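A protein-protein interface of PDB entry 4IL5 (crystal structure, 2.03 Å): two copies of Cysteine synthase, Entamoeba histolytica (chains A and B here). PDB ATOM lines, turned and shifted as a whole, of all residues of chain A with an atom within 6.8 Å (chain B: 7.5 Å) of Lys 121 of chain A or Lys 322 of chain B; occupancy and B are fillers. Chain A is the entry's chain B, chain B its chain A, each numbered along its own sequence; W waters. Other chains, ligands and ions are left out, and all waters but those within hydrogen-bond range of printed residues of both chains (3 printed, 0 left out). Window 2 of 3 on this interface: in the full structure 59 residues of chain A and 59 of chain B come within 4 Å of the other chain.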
ATOM      1  N   CYS A  94     -26.613  -9.864  -9.011  1.00  0.00           N
ATOM      2  CA  CYS A  94     -25.485  -9.296  -8.250  1.00  0.00           C
ATOM      3  C   CYS A  94     -24.923  -7.989  -8.874  1.00  0.00           C
ATOM      4  O   CYS A  94     -24.627  -7.027  -8.162  1.00  0.00           O
ATOM      5  CB  CYS A  94     -24.363 -10.324  -8.137  1.00  0.00           C
ATOM      6  SG  CYS A  94     -24.770 -11.836  -7.229  1.00  0.00           S
ATOM      7  N   ARG A 116     -19.022 -19.867 -10.163  1.00  0.00           N
ATOM      8  CA  ARG A 116     -20.088 -18.842 -10.209  1.00  0.00           C
ATOM      9  C   ARG A 116     -20.383 -18.327  -8.799  1.00  0.00           C
ATOM     10  O   ARG A 116     -20.657 -17.145  -8.620  1.00  0.00           O
ATOM     11  CB  ARG A 116     -21.358 -19.307 -10.920  1.00  0.00           C
ATOM     12  CG  ARG A 116     -21.332 -19.144 -12.433  1.00  0.00           C
ATOM     13  CD  ARG A 116     -22.753 -19.071 -12.984  1.00  0.00           C
ATOM     14  NE  ARG A 116     -22.834 -19.274 -14.434  1.00  0.00           N
ATOM     15  CZ  ARG A 116     -22.961 -20.464 -15.017  1.00  0.00           C
ATOM     16  NH1 ARG A 116     -23.004 -21.565 -14.272  1.00  0.00           N
ATOM     17  NH2 ARG A 116     -23.034 -20.557 -16.346  1.00  0.00           N
ATOM     18  N   GLN A 117     -20.265 -19.212  -7.808  1.00  0.00           N
ATOM     19  CA  GLN A 117     -20.296 -18.799  -6.408  1.00  0.00           C
ATOM     20  C   GLN A 117     -19.282 -17.699  -6.121  1.00  0.00           C
ATOM     21  O   GLN A 117     -19.625 -16.661  -5.549  1.00  0.00           O
ATOM     22  CB  GLN A 117     -20.028 -19.988  -5.492  1.00  0.00           C
ATOM     23  CG  GLN A 117     -21.089 -21.065  -5.589  1.00  0.00           C
ATOM     24  CD  GLN A 117     -20.919 -22.170  -4.564  1.00  0.00           C
ATOM     25  OE1 GLN A 117     -20.284 -21.988  -3.517  1.00  0.00           O
ATOM     26  NE2 GLN A 117     -21.500 -23.329  -4.862  1.00  0.00           N
ATOM     27  N   MET A 118     -18.032 -17.930  -6.523  1.00  0.00           N
ATOM     28  CA  MET A 118     -16.981 -16.909  -6.367  1.00  0.00           C
ATOM     29  C   MET A 118     -17.351 -15.593  -7.085  1.00  0.00           C
ATOM     30  O   MET A 118     -17.168 -14.512  -6.512  1.00  0.00           O
ATOM     31  CB  MET A 118     -15.620 -17.433  -6.846  1.00  0.00           C
ATOM     32  CG  MET A 118     -14.444 -16.483  -6.623  1.00  0.00           C
ATOM     33  SD  MET A 118     -12.878 -17.047  -7.354  1.00  0.00           S
ATOM     34  CE  MET A 118     -13.021 -18.828  -7.043  1.00  0.00           C
ATOM     35  N   ILE A 119     -17.864 -15.688  -8.321  1.00  0.00           N
ATOM     36  CA  ILE A 119     -18.316 -14.489  -9.065  1.00  0.00           C
ATOM     37  C   ILE A 119     -19.354 -13.753  -8.235  1.00  0.00           C
ATOM     38  O   ILE A 119     -19.216 -12.571  -7.932  1.00  0.00           O
ATOM     39  CB  ILE A 119     -18.869 -14.805 -10.483  1.00  0.00           C
ATOM     40  CG1 ILE A 119     -17.778 -15.459 -11.353  1.00  0.00           C
ATOM     41  CG2 ILE A 119     -19.434 -13.528 -11.148  1.00  0.00           C
ATOM     42  CD1 ILE A 119     -18.185 -15.780 -12.776  1.00  0.00           C
ATOM     43  N   MET A 120     -20.356 -14.479  -7.784  1.00  0.00           N
ATOM     44  CA  MET A 120     -21.414 -13.849  -7.010  1.00  0.00           C
ATOM     45  C   MET A 120     -20.927 -13.241  -5.688  1.00  0.00           C
ATOM     46  O   MET A 120     -21.323 -12.114  -5.337  1.00  0.00           O
ATOM     47  CB  MET A 120     -22.599 -14.801  -6.883  1.00  0.00           C
ATOM     48  CG  MET A 120     -23.211 -15.124  -8.254  1.00  0.00           C
ATOM     49  SD  MET A 120     -24.628 -16.201  -8.078  1.00  0.00           S
ATOM     50  CE  MET A 120     -24.397 -17.363  -9.433  1.00  0.00           C
ATOM     51  N   LYS A 121     -20.027 -13.941  -4.989  1.00  0.00           N
ATOM     52  CA  LYS A 121     -19.380 -13.351  -3.783  1.00  0.00           C
ATOM     53  C   LYS A 121     -18.537 -12.106  -4.076  1.00  0.00           C
ATOM     54  O   LYS A 121     -18.610 -11.113  -3.346  1.00  0.00           O
ATOM     55  CB  LYS A 121     -18.536 -14.380  -3.023  1.00  0.00           C
ATOM     56  CG  LYS A 121     -19.378 -15.374  -2.230  1.00  0.00           C
ATOM     57  CD  LYS A 121     -18.574 -16.602  -1.788  1.00  0.00           C
ATOM     58  CE  LYS A 121     -18.192 -16.530  -0.313  1.00  0.00           C
ATOM     59  NZ  LYS A 121     -17.114 -17.505   0.035  1.00  0.00           N
ATOM     60  N   ALA A 122     -17.749 -12.146  -5.150  1.00  0.00           N
ATOM     61  CA  ALA A 122     -16.959 -10.972  -5.564  1.00  0.00           C
ATOM     62  C   ALA A 122     -17.860  -9.730  -5.671  1.00  0.00           C
ATOM     63  O   ALA A 122     -17.459  -8.611  -5.333  1.00  0.00           O
ATOM     64  CB  ALA A 122     -16.271 -11.260  -6.887  1.00  0.00           C
ATOM     65  N   PHE A 123     -19.096  -9.935  -6.135  1.00  0.00           N
ATOM     66  CA  PHE A 123     -20.058  -8.833  -6.245  1.00  0.00           C
ATOM     67  C   PHE A 123     -20.658  -8.414  -4.910  1.00  0.00           C
ATOM     68  O   PHE A 123     -21.413  -7.448  -4.839  1.00  0.00           O
ATOM     69  CB  PHE A 123     -21.167  -9.182  -7.244  1.00  0.00           C
ATOM     70  CG  PHE A 123     -20.812  -8.882  -8.679  1.00  0.00           C
ATOM     71  CD1 PHE A 123     -21.062  -7.626  -9.218  1.00  0.00           C
ATOM     72  CD2 PHE A 123     -20.254  -9.862  -9.491  1.00  0.00           C
ATOM     73  CE1 PHE A 123     -20.763  -7.351 -10.547  1.00  0.00           C
ATOM     74  CE2 PHE A 123     -19.929  -9.588 -10.826  1.00  0.00           C
ATOM     75  CZ  PHE A 123     -20.180  -8.332 -11.351  1.00  0.00           C
ATOM     76  N   GLY A 124     -20.322  -9.145  -3.858  1.00  0.00           N
ATOM     77  CA  GLY A 124     -20.796  -8.833  -2.519  1.00  0.00           C
ATOM     78  C   GLY A 124     -22.069  -9.587  -2.189  1.00  0.00           C
ATOM     79  O   GLY A 124     -22.720  -9.282  -1.207  1.00  0.00           O
ATOM     80  N   ALA A 125     -22.433 -10.578  -2.997  1.00  0.00           N
ATOM     81  CA  ALA A 125     -23.638 -11.347  -2.691  1.00  0.00           C
ATOM     82  C   ALA A 125     -23.449 -12.200  -1.435  1.00  0.00           C
ATOM     83  O   ALA A 125     -22.352 -12.697  -1.159  1.00  0.00           O
ATOM     84  CB  ALA A 125     -24.059 -12.228  -3.856  1.00  0.00           C
ATOM     85  N   GLU A 126     -24.533 -12.336  -0.681  1.00  0.00           N
ATOM     86  CA  GLU A 126     -24.668 -13.391   0.318  1.00  0.00           C
ATOM     87  C   GLU A 126     -25.151 -14.649  -0.391  1.00  0.00           C
ATOM     88  O   GLU A 126     -26.188 -14.621  -1.067  1.00  0.00           O
ATOM     89  CB  GLU A 126     -25.715 -12.978   1.348  1.00  0.00           C
ATOM     90  CG  GLU A 126     -26.113 -14.079   2.302  1.00  0.00           C
ATOM     91  CD  GLU A 126     -25.520 -13.855   3.672  1.00  0.00           C
ATOM     92  OE1 GLU A 126     -24.271 -13.765   3.784  1.00  0.00           O
ATOM     93  OE2 GLU A 126     -26.315 -13.734   4.629  1.00  0.00           O
ATOM     94  N   LEU A 127     -24.419 -15.749  -0.225  1.00  0.00           N
ATOM     95  CA  LEU A 127     -24.819 -17.029  -0.786  1.00  0.00           C
ATOM     96  C   LEU A 127     -25.538 -17.897   0.228  1.00  0.00           C
ATOM     97  O   LEU A 127     -25.159 -17.944   1.393  1.00  0.00           O
ATOM     98  CB  LEU A 127     -23.598 -17.793  -1.275  1.00  0.00           C
ATOM     99  CG  LEU A 127     -22.838 -17.188  -2.451  1.00  0.00           C
ATOM    100  CD1 LEU A 127     -21.810 -18.210  -2.904  1.00  0.00           C
ATOM    101  CD2 LEU A 127     -23.775 -16.822  -3.601  1.00  0.00           C
ATOM    102  N   ARG B 267     -11.094  -5.749  -6.188  1.00  0.00           N
ATOM    103  CA  ARG B 267     -12.191  -6.218  -5.344  1.00  0.00           C
ATOM    104  C   ARG B 267     -13.165  -5.101  -5.008  1.00  0.00           C
ATOM    105  O   ARG B 267     -14.403  -5.322  -5.006  1.00  0.00           O
ATOM    106  CB  ARG B 267     -11.671  -6.901  -4.060  1.00  0.00           C
ATOM    107  CG  ARG B 267     -11.131  -8.300  -4.296  1.00  0.00           C
ATOM    108  CD  ARG B 267     -10.874  -9.045  -2.984  1.00  0.00           C
ATOM    109  NE  ARG B 267     -10.000  -8.303  -2.050  1.00  0.00           N
ATOM    110  CZ  ARG B 267      -8.671  -8.431  -1.986  1.00  0.00           C
ATOM    111  NH1 ARG B 267      -8.024  -9.233  -2.823  1.00  0.00           N
ATOM    112  NH2 ARG B 267      -7.990  -7.746  -1.079  1.00  0.00           N
ATOM    113  N   VAL B 270     -15.424  -4.069  -8.216  1.00  0.00           N
ATOM    114  CA  VAL B 270     -16.578  -4.932  -8.514  1.00  0.00           C
ATOM    115  C   VAL B 270     -17.670  -4.744  -7.464  1.00  0.00           C
ATOM    116  O   VAL B 270     -18.860  -4.615  -7.799  1.00  0.00           O
ATOM    117  CB  VAL B 270     -16.196  -6.415  -8.772  1.00  0.00           C
ATOM    118  CG1 VAL B 270     -15.658  -7.107  -7.532  1.00  0.00           C
ATOM    119  CG2 VAL B 270     -17.369  -7.199  -9.345  1.00  0.00           C
ATOM    120  N   LYS B 271     -17.261  -4.661  -6.201  1.00  0.00           N
ATOM    121  CA  LYS B 271     -18.230  -4.600  -5.104  1.00  0.00           C
ATOM    122  C   LYS B 271     -18.986  -3.255  -5.054  1.00  0.00           C
ATOM    123  O   LYS B 271     -20.204  -3.227  -4.796  1.00  0.00           O
ATOM    124  CB  LYS B 271     -17.519  -4.924  -3.789  1.00  0.00           C
ATOM    125  CG  LYS B 271     -18.375  -4.826  -2.539  1.00  0.00           C
ATOM    126  CD  LYS B 271     -17.660  -5.495  -1.361  1.00  0.00           C
ATOM    127  CE  LYS B 271     -18.485  -5.314  -0.097  1.00  0.00           C
ATOM    128  NZ  LYS B 271     -17.997  -6.176   1.006  1.00  0.00           N
ATOM    129  N   ASP B 317      -5.698 -15.858  -6.563  1.00  0.00           N
ATOM    130  CA  ASP B 317      -6.101 -15.383  -5.237  1.00  0.00           C
ATOM    131  C   ASP B 317      -6.848 -14.040  -5.250  1.00  0.00           C
ATOM    132  O   ASP B 317      -7.042 -13.420  -4.208  1.00  0.00           O
ATOM    133  CB  ASP B 317      -4.875 -15.258  -4.334  1.00  0.00           C
ATOM    134  CG  ASP B 317      -4.320 -16.612  -3.889  1.00  0.00           C
ATOM    135  OD1 ASP B 317      -5.009 -17.644  -4.066  1.00  0.00           O
ATOM    136  OD2 ASP B 317      -3.192 -16.619  -3.355  1.00  0.00           O
ATOM    137  N   LEU B 318      -7.236 -13.571  -6.427  1.00  0.00           N
ATOM    138  CA  LEU B 318      -7.821 -12.230  -6.534  1.00  0.00           C
ATOM    139  C   LEU B 318      -8.987 -12.050  -5.565  1.00  0.00           C
ATOM    140  O   LEU B 318      -8.980 -11.088  -4.783  1.00  0.00           O
ATOM    141  CB  LEU B 318      -8.227 -11.903  -7.994  1.00  0.00           C
ATOM    142  CG  LEU B 318      -9.044 -10.634  -8.285  1.00  0.00           C
ATOM    143  CD1 LEU B 318      -8.367  -9.367  -7.737  1.00  0.00           C
ATOM    144  CD2 LEU B 318      -9.305 -10.523  -9.793  1.00  0.00           C
ATOM    145  N   TYR B 319      -9.953 -12.981  -5.608  1.00  0.00           N
ATOM    146  CA  TYR B 319     -11.145 -12.899  -4.772  1.00  0.00           C
ATOM    147  C   TYR B 319     -11.106 -13.818  -3.549  1.00  0.00           C
ATOM    148  O   TYR B 319     -12.096 -13.925  -2.826  1.00  0.00           O
ATOM    149  CB  TYR B 319     -12.427 -13.185  -5.588  1.00  0.00           C
ATOM    150  CG  TYR B 319     -12.572 -12.300  -6.812  1.00  0.00           C
ATOM    151  CD1 TYR B 319     -12.786 -10.926  -6.675  1.00  0.00           C
ATOM    152  CD2 TYR B 319     -12.489 -12.834  -8.102  1.00  0.00           C
ATOM    153  CE1 TYR B 319     -12.913 -10.104  -7.781  1.00  0.00           C
ATOM    154  CE2 TYR B 319     -12.621 -12.017  -9.223  1.00  0.00           C
ATOM    155  CZ  TYR B 319     -12.831 -10.654  -9.047  1.00  0.00           C
ATOM    156  OH  TYR B 319     -12.959  -9.838 -10.133  1.00  0.00           O
ATOM    157  N   LYS B 320      -9.982 -14.484  -3.301  1.00  0.00           N
ATOM    158  CA  LYS B 320      -9.946 -15.400  -2.163  1.00  0.00           C
ATOM    159  C   LYS B 320      -9.825 -14.605  -0.845  1.00  0.00           C
ATOM    160  O   LYS B 320     -10.539 -14.855   0.130  1.00  0.00           O
ATOM    161  CB  LYS B 320      -8.874 -16.477  -2.374  1.00  0.00           C
ATOM    162  CG  LYS B 320      -9.038 -17.218  -3.712  1.00  0.00           C
ATOM    163  CD  LYS B 320      -8.462 -18.634  -3.686  1.00  0.00           C
ATOM    164  CE  LYS B 320      -8.026 -19.122  -5.061  1.00  0.00           C
ATOM    165  NZ  LYS B 320      -9.144 -19.506  -5.972  1.00  0.00           N
ATOM    166  N   ILE B 321      -8.992 -13.577  -0.869  1.00  0.00           N
ATOM    167  CA  ILE B 321      -8.786 -12.690   0.262  1.00  0.00           C
ATOM    168  C   ILE B 321     -10.016 -11.779   0.429  1.00  0.00           C
ATOM    169  O   ILE B 321     -10.399 -11.067  -0.507  1.00  0.00           O
ATOM    170  CB  ILE B 321      -7.467 -11.890   0.038  1.00  0.00           C
ATOM    171  CG1 ILE B 321      -6.337 -12.852  -0.434  1.00  0.00           C
ATOM    172  CG2 ILE B 321      -7.106 -11.079   1.275  1.00  0.00           C
ATOM    173  CD1 ILE B 321      -5.079 -12.215  -1.016  1.00  0.00           C
ATOM    174  N   LYS B 322     -10.671 -11.819   1.592  1.00  0.00           N
ATOM    175  CA  LYS B 322     -11.896 -11.017   1.792  1.00  0.00           C
ATOM    176  C   LYS B 322     -11.657  -9.851   2.737  1.00  0.00           C
ATOM    177  O   LYS B 322     -11.174 -10.043   3.853  1.00  0.00           O
ATOM    178  CB  LYS B 322     -13.064 -11.861   2.291  1.00  0.00           C
ATOM    179  CG  LYS B 322     -13.549 -12.895   1.287  1.00  0.00           C
ATOM    180  CD  LYS B 322     -14.640 -12.360   0.367  1.00  0.00           C
ATOM    181  CE  LYS B 322     -15.333 -13.498  -0.370  1.00  0.00           C
ATOM    182  NZ  LYS B 322     -16.041 -14.390   0.596  1.00  0.00           N
ATOM    183  N   ASP B 323     -11.993  -8.645   2.284  1.00  0.00           N
ATOM    184  CA  ASP B 323     -11.643  -7.432   3.016  1.00  0.00           C
ATOM    185  C   ASP B 323     -12.657  -7.153   4.110  1.00  0.00           C
ATOM    186  O   ASP B 323     -13.861  -7.120   3.860  1.00  0.00           O
ATOM    187  CB  ASP B 323     -11.535  -6.230   2.065  1.00  0.00           C
ATOM    188  CG  ASP B 323     -10.580  -6.485   0.909  1.00  0.00           C
ATOM    189  OD1 ASP B 323      -9.359  -6.628   1.157  1.00  0.00           O
ATOM    190  OD2 ASP B 323     -11.056  -6.562  -0.251  1.00  0.00           O
ATOM    191  N   GLU B 324     -12.174  -6.967   5.331  1.00  0.00           N
ATOM    192  CA  GLU B 324     -13.051  -6.528   6.412  1.00  0.00           C
ATOM    193  C   GLU B 324     -13.176  -5.012   6.341  1.00  0.00           C
ATOM    194  O   GLU B 324     -12.239  -4.325   5.962  1.00  0.00           O
ATOM    195  CB  GLU B 324     -12.495  -6.956   7.770  1.00  0.00           C
ATOM    196  CG  GLU B 324     -12.561  -8.458   8.023  1.00  0.00           C
ATOM    197  CD  GLU B 324     -11.555  -8.929   9.067  1.00  0.00           C
ATOM    198  OE1 GLU B 324     -11.255  -8.167  10.017  1.00  0.00           O
ATOM    199  OE2 GLU B 324     -11.061 -10.071   8.938  1.00  0.00           O
ATOM    200  N   GLY B 325     -14.341  -4.489   6.680  1.00  0.00           N
ATOM    201  CA  GLY B 325     -14.509  -3.053   6.739  1.00  0.00           C
ATOM    202  C   GLY B 325     -15.490  -2.536   5.724  1.00  0.00           C
ATOM    203  O   GLY B 325     -15.773  -3.186   4.717  1.00  0.00           O
ATOM    204  N   ILE B 330     -12.217   0.718   3.317  1.00  0.00           N
ATOM    205  CA  ILE B 330     -11.493   0.109   2.206  1.00  0.00           C
ATOM    206  C   ILE B 330     -10.837   1.171   1.345  1.00  0.00           C
ATOM    207  O   ILE B 330      -9.669   1.076   1.037  1.00  0.00           O
ATOM    208  CB  ILE B 330     -12.445  -0.748   1.331  1.00  0.00           C
ATOM    209  CG1 ILE B 330     -13.087  -1.847   2.172  1.00  0.00           C
ATOM    210  CG2 ILE B 330     -11.704  -1.341   0.126  1.00  0.00           C
ATOM    211  CD1 ILE B 330     -12.099  -2.849   2.682  1.00  0.00           C
HETATM  212  O   HOH W   1     -21.779  -4.997  -3.721  1.00  0.00           O
HETATM  213  O   HOH W   2     -15.045  -7.975  -4.441  1.00  0.00           O
HETATM  214  O   HOH W   3      -9.941 -15.350  -7.107  1.00  0.00           O
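Water W1 lies within hydrogen-bond range of the backbone carbonyl oxygen (O) of Lys 271 of chain B (2.6 Å) and the backbone carbonyl oxygen (O) of Phe 123 of chain A (2.7 Å).
Water W2 bridges the backbone carbonyl oxygen of Ala 122 of chain A (2.7 Å) and the backbone carbonyl oxygen of Arg 267 of chain B (2.8 Å).
Water W3 lies within hydrogen-bond range of the backbone NH of Tyr 319 of chain B (2.8 Å), the backbone NH of Leu 318 of chain B (3.3 Å) and the side-chain sulfur of Met 118 of chain A (3.4 Å).
Of chain B, only Lys 322 comes within 4 Å of Lys 121 of chain A.
Of the printed residues of chain B, Ala 122 of chain A touches Val 270 (3.2 Å), Lys 271 (3.998 Å) and Tyr 319 (3.5 Å).
Printed residues of chain B within 4 Å of Phe 123 of chain A: Val 270.
Of the printed residues of chain A, Val 270 of chain B touches Ala 122 and Phe 123.
Printed residues of chain A within 4 Å of Lys 271 of chain B: Ala 122 (3.998 Å).
The nearest printed residue of chain A that does not touch Val 270 of chain B is Ile 119 of chain A (5.9 Å).
No position is printed for both chains.
Of the 5 pairs that touch across the chains among the printed residues, none has its exchanged pair printed and touching as well.
Among the printed residues, pairs that only touch across the chains: Ala 122 of chain A with Val 270 of chain B (3.2 Å), Ala 122 of chain A with Lys 271 of chain B (3.998 Å), Ala 122 of chain A with Tyr 319 of chain B (3.5 Å) and Phe 123 of chain A with Val 270 of chain B (3.6 Å).
The side-chain amino group (NZ) of Lys 322 of chain B lies close to the side-chain amino group (NZ) of Lys 121 of chain A (3.3 Å).
Of the 13 printed residues of chain A, 3 touch a printed residue of chain B.
Of the 13 printed residues of chain B, 4 touch a printed residue of chain A.
Hydrophobic or aromatic side chains of chain B that line the printed part of chain A: Val 270 and Tyr 319.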
